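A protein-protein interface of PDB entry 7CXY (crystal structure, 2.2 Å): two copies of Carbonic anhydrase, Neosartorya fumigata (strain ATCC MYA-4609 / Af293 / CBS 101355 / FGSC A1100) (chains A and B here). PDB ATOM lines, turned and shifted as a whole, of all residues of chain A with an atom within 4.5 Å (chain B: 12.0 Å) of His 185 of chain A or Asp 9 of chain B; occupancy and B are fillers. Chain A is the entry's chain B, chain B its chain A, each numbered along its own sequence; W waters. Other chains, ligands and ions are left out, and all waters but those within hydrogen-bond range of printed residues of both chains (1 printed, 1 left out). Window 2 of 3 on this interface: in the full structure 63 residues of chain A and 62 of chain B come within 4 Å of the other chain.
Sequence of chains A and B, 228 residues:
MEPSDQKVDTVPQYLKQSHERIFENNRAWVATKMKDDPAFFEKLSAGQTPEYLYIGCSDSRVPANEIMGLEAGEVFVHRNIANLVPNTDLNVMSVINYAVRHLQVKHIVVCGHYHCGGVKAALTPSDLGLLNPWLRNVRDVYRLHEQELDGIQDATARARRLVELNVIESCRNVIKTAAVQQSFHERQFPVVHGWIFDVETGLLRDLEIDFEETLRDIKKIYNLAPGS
NE2 of Gln 188 of chain A lies within hydrogen-bond range of O of His 185 of chain A, at 3.0 Å.
OD2 of Asp 9 of chain B lies within hydrogen-bond range of ND1 of His 185 of chain A (3.4 Å).
Hydrophobic or aromatic side chains of chain B that line the printed part of chain A: Val 11, Pro 12 and Leu 15.
Hydrophobic or aromatic side chains of chain A within 4 Å of the printed part of chain B: Phe 184 and His 185.
Among the printed residues, 6 pairs touch across the chains.
Among the printed residues, no Asp or Glu carboxylate lies within 4 Å of a Lys or Arg side-chain nitrogen of the other chain.
Water W1 lies within hydrogen-bond range of the side-chain hydroxyl of Tyr 14 of chain B (2.8 Å), the backbone carbonyl oxygen of Arg 187 of chain A (3.2 Å) and the backbone carbonyl oxygen of Gln 188 of chain A (3.3 Å).
Phe 184 of chain A touches Asp 9 of chain B.
O of Thr 10 of chain B touches CZ of Phe 184 of chain A, 3.7 Å away.
Pro 12 of chain B touches Gln 188 of chain A.
Leu 15 of chain B touches Gln 188 of chain A.
OE2 of Glu 212 of chain A touches CG2 of Val 11 of chain B, at 3.9 Å.
No position is printed for both chains.
Of the 6 pairs that touch across the chains among the printed residues, none has its exchanged pair printed and touching as well.
Gln 181 of chain A touches none of the printed residues of chain B.
Phe 184 of chain A touches just these residues of chain B: Asp 9 and Thr 10.
Of chain B, only Asp 9 (3.4 Å) comes within 4 Å of His 185 of chain A.
Arg 187 of chain A touches none of the printed residues of chain B.
Of chain B, only Pro 12 and Leu 15 come within 4 Å of Gln 188 of chain A.
Of chain B, only Val 11 comes within 4 Å of Glu 212 of chain A.
Of chain A, only Phe 184 and His 185 come within 4 Å of Asp 9 of chain B.
Printed residues of chain A within 4 Å of Thr 10 of chain B: Phe 184 (3.7 Å).
Of the printed residues of chain A, Pro 12 of chain B touches Gln 188 (3.7 Å).
The nearest residue of chain B that does not touch His 185 of chain A is Thr 10 of chain B (8.2 Å).
The nearest printed residue of chain A that does not touch Thr 10 of chain B is Gln 188 of chain A (4.3 Å).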
ATOM      1  N   GLN A 181     -26.828 -10.724  -4.676  1.00  0.00           N
ATOM      2  CA  GLN A 181     -27.065 -12.058  -5.278  1.00  0.00           C
ATOM      3  C   GLN A 181     -25.774 -12.564  -5.932  1.00  0.00           C
ATOM      4  O   GLN A 181     -25.384 -13.693  -5.635  1.00  0.00           O
ATOM      5  CB  GLN A 181     -28.211 -11.999  -6.287  1.00  0.00           C
ATOM      6  CG  GLN A 181     -29.569 -12.166  -5.641  1.00  0.00           C
ATOM      7  CD  GLN A 181     -30.652 -11.913  -6.654  1.00  0.00           C
ATOM      8  OE1 GLN A 181     -30.636 -12.468  -7.744  1.00  0.00           O
ATOM      9  NE2 GLN A 181     -31.580 -11.037  -6.322  1.00  0.00           N
ATOM     10  N   GLN A 182     -25.112 -11.751  -6.749  1.00  0.00           N
ATOM     11  CA  GLN A 182     -23.901 -12.198  -7.484  1.00  0.00           C
ATOM     12  C   GLN A 182     -22.777 -12.433  -6.488  1.00  0.00           C
ATOM     13  O   GLN A 182     -22.177 -13.502  -6.552  1.00  0.00           O
ATOM     14  CB  GLN A 182     -23.540 -11.231  -8.604  1.00  0.00           C
ATOM     15  CG  GLN A 182     -24.520 -11.380  -9.762  1.00  0.00           C
ATOM     16  CD  GLN A 182     -24.285 -10.433 -10.911  1.00  0.00           C
ATOM     17  OE1 GLN A 182     -23.631  -9.400 -10.772  1.00  0.00           O
ATOM     18  NE2 GLN A 182     -24.837 -10.793 -12.058  1.00  0.00           N
ATOM     19  N   SER A 183     -22.552 -11.506  -5.562  1.00  0.00           N
ATOM     20  CA  SER A 183     -21.507 -11.644  -4.525  1.00  0.00           C
ATOM     21  C   SER A 183     -21.793 -12.896  -3.704  1.00  0.00           C
ATOM     22  O   SER A 183     -20.833 -13.614  -3.418  1.00  0.00           O
ATOM     23  CB  SER A 183     -21.418 -10.434  -3.639  1.00  0.00           C
ATOM     24  OG  SER A 183     -20.489 -10.628  -2.579  1.00  0.00           O
ATOM     25  N   PHE A 184     -23.045 -13.127  -3.278  1.00  0.00           N
ATOM     26  CA  PHE A 184     -23.316 -14.278  -2.389  1.00  0.00           C
ATOM     27  C   PHE A 184     -23.082 -15.591  -3.160  1.00  0.00           C
ATOM     28  O   PHE A 184     -22.518 -16.532  -2.572  1.00  0.00           O
ATOM     29  CB  PHE A 184     -24.696 -14.236  -1.756  1.00  0.00           C
ATOM     30  CG  PHE A 184     -24.837 -15.338  -0.748  1.00  0.00           C
ATOM     31  CD1 PHE A 184     -24.302 -15.199   0.516  1.00  0.00           C
ATOM     32  CD2 PHE A 184     -25.368 -16.565  -1.103  1.00  0.00           C
ATOM     33  CE1 PHE A 184     -24.354 -16.233   1.434  1.00  0.00           C
ATOM     34  CE2 PHE A 184     -25.449 -17.588  -0.173  1.00  0.00           C
ATOM     35  CZ  PHE A 184     -24.935 -17.425   1.090  1.00  0.00           C
ATOM     36  N   HIS A 185     -23.453 -15.639  -4.439  1.00  0.00           N
ATOM     37  CA  HIS A 185     -23.266 -16.823  -5.314  1.00  0.00           C
ATOM     38  C   HIS A 185     -21.769 -17.110  -5.453  1.00  0.00           C
ATOM     39  O   HIS A 185     -21.366 -18.261  -5.231  1.00  0.00           O
ATOM     40  CB  HIS A 185     -23.928 -16.610  -6.679  1.00  0.00           C
ATOM     41  CG  HIS A 185     -23.944 -17.828  -7.548  1.00  0.00           C
ATOM     42  ND1 HIS A 185     -24.656 -18.981  -7.211  1.00  0.00           N
ATOM     43  CD2 HIS A 185     -23.372 -18.073  -8.749  1.00  0.00           C
ATOM     44  CE1 HIS A 185     -24.504 -19.882  -8.159  1.00  0.00           C
ATOM     45  NE2 HIS A 185     -23.727 -19.346  -9.116  1.00  0.00           N
ATOM     46  N   GLU A 186     -20.972 -16.091  -5.777  1.00  0.00           N
ATOM     47  CA  GLU A 186     -19.546 -16.259  -6.152  1.00  0.00           C
ATOM     48  C   GLU A 186     -18.655 -16.413  -4.922  1.00  0.00           C
ATOM     49  O   GLU A 186     -17.577 -16.940  -5.112  1.00  0.00           O
ATOM     50  CB  GLU A 186     -19.027 -15.086  -6.979  1.00  0.00           C
ATOM     51  CG  GLU A 186     -19.478 -15.149  -8.427  1.00  0.00           C
ATOM     52  CD  GLU A 186     -19.355 -13.841  -9.187  1.00  0.00           C
ATOM     53  OE1 GLU A 186     -18.477 -13.013  -8.817  1.00  0.00           O
ATOM     54  OE2 GLU A 186     -20.126 -13.660 -10.160  1.00  0.00           O
ATOM     55  N   ARG A 187     -19.050 -15.930  -3.743  1.00  0.00           N
ATOM     56  CA  ARG A 187     -18.106 -15.672  -2.617  1.00  0.00           C
ATOM     57  C   ARG A 187     -18.724 -15.954  -1.253  1.00  0.00           C
ATOM     58  O   ARG A 187     -18.004 -15.825  -0.276  1.00  0.00           O
ATOM     59  CB  ARG A 187     -17.651 -14.203  -2.625  1.00  0.00           C
ATOM     60  CG  ARG A 187     -17.094 -13.720  -3.961  1.00  0.00           C
ATOM     61  CD  ARG A 187     -16.461 -12.336  -3.920  1.00  0.00           C
ATOM     62  NE  ARG A 187     -17.402 -11.296  -3.532  1.00  0.00           N
ATOM     63  CZ  ARG A 187     -17.191  -9.984  -3.661  1.00  0.00           C
ATOM     64  NH1 ARG A 187     -16.053  -9.548  -4.179  1.00  0.00           N
ATOM     65  NH2 ARG A 187     -18.110  -9.112  -3.264  1.00  0.00           N
ATOM     66  N   GLN A 188     -20.016 -16.262  -1.184  1.00  0.00           N
ATOM     67  CA  GLN A 188     -20.729 -16.657   0.064  1.00  0.00           C
ATOM     68  C   GLN A 188     -20.745 -15.504   1.082  1.00  0.00           C
ATOM     69  O   GLN A 188     -20.860 -15.780   2.294  1.00  0.00           O
ATOM     70  CB  GLN A 188     -20.146 -17.982   0.601  1.00  0.00           C
ATOM     71  CG  GLN A 188     -20.439 -19.206  -0.283  1.00  0.00           C
ATOM     72  CD  GLN A 188     -19.601 -19.226  -1.545  1.00  0.00           C
ATOM     73  OE1 GLN A 188     -18.376 -19.047  -1.523  1.00  0.00           O
ATOM     74  NE2 GLN A 188     -20.258 -19.401  -2.683  1.00  0.00           N
ATOM     75  N   GLU A 212     -31.227 -17.240   3.471  1.00  0.00           N
ATOM     76  CA  GLU A 212     -31.024 -18.348   2.496  1.00  0.00           C
ATOM     77  C   GLU A 212     -32.376 -18.688   1.875  1.00  0.00           C
ATOM     78  O   GLU A 212     -32.466 -18.769   0.628  1.00  0.00           O
ATOM     79  CB  GLU A 212     -30.300 -19.541   3.151  1.00  0.00           C
ATOM     80  CG  GLU A 212     -30.776 -19.939   4.568  1.00  0.00           C
ATOM     81  CD  GLU A 212     -30.331 -19.119   5.793  1.00  0.00           C
ATOM     82  OE1 GLU A 212     -30.808 -17.968   5.955  1.00  0.00           O
ATOM     83  OE2 GLU A 212     -29.534 -19.643   6.625  1.00  0.00           O
ATOM     84  N   LYS A 219     -34.861 -16.040  -6.316  1.00  0.00           N
ATOM     85  CA  LYS A 219     -34.178 -16.621  -7.507  1.00  0.00           C
ATOM     86  C   LYS A 219     -35.122 -17.528  -8.312  1.00  0.00           C
ATOM     87  O   LYS A 219     -34.720 -17.926  -9.420  1.00  0.00           O
ATOM     88  CB  LYS A 219     -32.970 -17.457  -7.079  1.00  0.00           C
ATOM     89  CG  LYS A 219     -31.717 -16.690  -6.673  1.00  0.00           C
ATOM     90  CD  LYS A 219     -30.571 -17.618  -6.321  1.00  0.00           C
ATOM     91  CE  LYS A 219     -29.287 -16.876  -6.047  1.00  0.00           C
ATOM     92  NZ  LYS A 219     -28.689 -16.359  -7.302  1.00  0.00           N
ATOM     93  N   ASP B   9     -26.998 -22.449  -2.007  1.00  0.00           N
ATOM     94  CA  ASP B   9     -25.959 -21.496  -1.471  1.00  0.00           C
ATOM     95  C   ASP B   9     -26.122 -21.399   0.060  1.00  0.00           C
ATOM     96  O   ASP B   9     -27.060 -20.678   0.514  1.00  0.00           O
ATOM     97  CB  ASP B   9     -26.087 -20.099  -2.107  1.00  0.00           C
ATOM     98  CG  ASP B   9     -25.844 -19.946  -3.610  1.00  0.00           C
ATOM     99  OD1 ASP B   9     -25.146 -20.822  -4.178  1.00  0.00           O
ATOM    100  OD2 ASP B   9     -26.325 -18.907  -4.207  1.00  0.00           O
ATOM    101  N   THR B  10     -25.297 -22.093   0.856  1.00  0.00           N
ATOM    102  CA  THR B  10     -25.438 -22.083   2.347  1.00  0.00           C
ATOM    103  C   THR B  10     -24.639 -20.921   2.938  1.00  0.00           C
ATOM    104  O   THR B  10     -23.593 -20.575   2.355  1.00  0.00           O
ATOM    105  CB  THR B  10     -24.967 -23.360   3.056  1.00  0.00           C
ATOM    106  OG1 THR B  10     -25.146 -24.486   2.198  1.00  0.00           O
ATOM    107  CG2 THR B  10     -25.702 -23.586   4.363  1.00  0.00           C
ATOM    108  N   VAL B  11     -25.114 -20.381   4.062  1.00  0.00           N
ATOM    109  CA  VAL B  11     -24.458 -19.291   4.828  1.00  0.00           C
ATOM    110  C   VAL B  11     -23.339 -19.910   5.664  1.00  0.00           C
ATOM    111  O   VAL B  11     -23.628 -20.645   6.615  1.00  0.00           O
ATOM    112  CB  VAL B  11     -25.453 -18.527   5.719  1.00  0.00           C
ATOM    113  CG1 VAL B  11     -24.779 -17.477   6.583  1.00  0.00           C
ATOM    114  CG2 VAL B  11     -26.562 -17.894   4.898  1.00  0.00           C
ATOM    115  N   PRO B  12     -22.058 -19.574   5.346  1.00  0.00           N
ATOM    116  CA  PRO B  12     -20.910 -19.886   6.200  1.00  0.00           C
ATOM    117  C   PRO B  12     -21.158 -19.617   7.685  1.00  0.00           C
ATOM    118  O   PRO B  12     -21.608 -18.558   8.002  1.00  0.00           O
ATOM    119  CB  PRO B  12     -19.870 -18.883   5.688  1.00  0.00           C
ATOM    120  CG  PRO B  12     -20.141 -18.818   4.211  1.00  0.00           C
ATOM    121  CD  PRO B  12     -21.647 -18.859   4.125  1.00  0.00           C
ATOM    122  N   GLN B  13     -20.804 -20.557   8.553  1.00  0.00           N
ATOM    123  CA  GLN B  13     -21.044 -20.466  10.016  1.00  0.00           C
ATOM    124  C   GLN B  13     -20.353 -19.230  10.600  1.00  0.00           C
ATOM    125  O   GLN B  13     -20.870 -18.689  11.597  1.00  0.00           O
ATOM    126  CB  GLN B  13     -20.579 -21.770  10.696  1.00  0.00           C
ATOM    127  CG  GLN B  13     -20.706 -21.797  12.226  1.00  0.00           C
ATOM    128  CD  GLN B  13     -22.125 -21.721  12.755  1.00  0.00           C
ATOM    129  OE1 GLN B  13     -23.063 -22.269  12.165  1.00  0.00           O
ATOM    130  NE2 GLN B  13     -22.294 -21.048  13.889  1.00  0.00           N
ATOM    131  N   TYR B  14     -19.199 -18.793  10.083  1.00  0.00           N
ATOM    132  CA  TYR B  14     -18.497 -17.628  10.690  1.00  0.00           C
ATOM    133  C   TYR B  14     -19.395 -16.371  10.608  1.00  0.00           C
ATOM    134  O   TYR B  14     -19.325 -15.512  11.509  1.00  0.00           O
ATOM    135  CB  TYR B  14     -17.115 -17.443  10.069  1.00  0.00           C
ATOM    136  CG  TYR B  14     -17.075 -16.697   8.766  1.00  0.00           C
ATOM    137  CD1 TYR B  14     -16.930 -15.317   8.736  1.00  0.00           C
ATOM    138  CD2 TYR B  14     -17.160 -17.365   7.570  1.00  0.00           C
ATOM    139  CE1 TYR B  14     -16.884 -14.630   7.534  1.00  0.00           C
ATOM    140  CE2 TYR B  14     -17.136 -16.691   6.362  1.00  0.00           C
ATOM    141  CZ  TYR B  14     -16.976 -15.318   6.346  1.00  0.00           C
ATOM    142  OH  TYR B  14     -16.934 -14.661   5.157  1.00  0.00           O
ATOM    143  N   LEU B  15     -20.248 -16.276   9.584  1.00  0.00           N
ATOM    144  CA  LEU B  15     -21.177 -15.119   9.411  1.00  0.00           C
ATOM    145  C   LEU B  15     -22.272 -15.170  10.479  1.00  0.00           C
ATOM    146  O   LEU B  15     -22.634 -14.107  10.978  1.00  0.00           O
ATOM    147  CB  LEU B  15     -21.710 -15.112   7.979  1.00  0.00           C
ATOM    148  CG  LEU B  15     -20.628 -14.860   6.939  1.00  0.00           C
ATOM    149  CD1 LEU B  15     -21.134 -15.078   5.530  1.00  0.00           C
ATOM    150  CD2 LEU B  15     -20.028 -13.468   7.078  1.00  0.00           C
ATOM    151  N   LYS B  16     -22.657 -16.360  10.944  1.00  0.00           N
ATOM    152  CA  LYS B  16     -23.646 -16.519  12.050  1.00  0.00           C
ATOM    153  C   LYS B  16     -23.013 -16.102  13.381  1.00  0.00           C
ATOM    154  O   LYS B  16     -23.707 -15.448  14.170  1.00  0.00           O
ATOM    155  CB  LYS B  16     -24.189 -17.948  12.065  1.00  0.00           C
ATOM    156  CG  LYS B  16     -24.796 -18.365  10.732  1.00  0.00           C
ATOM    157  CD  LYS B  16     -25.509 -19.693  10.716  1.00  0.00           C
ATOM    158  CE  LYS B  16     -25.992 -20.027   9.318  1.00  0.00           C
ATOM    159  NZ  LYS B  16     -26.742 -21.306   9.269  1.00  0.00           N
HETATM  160  O   HOH W   1     -17.658 -16.102   2.861  1.00  0.00           O
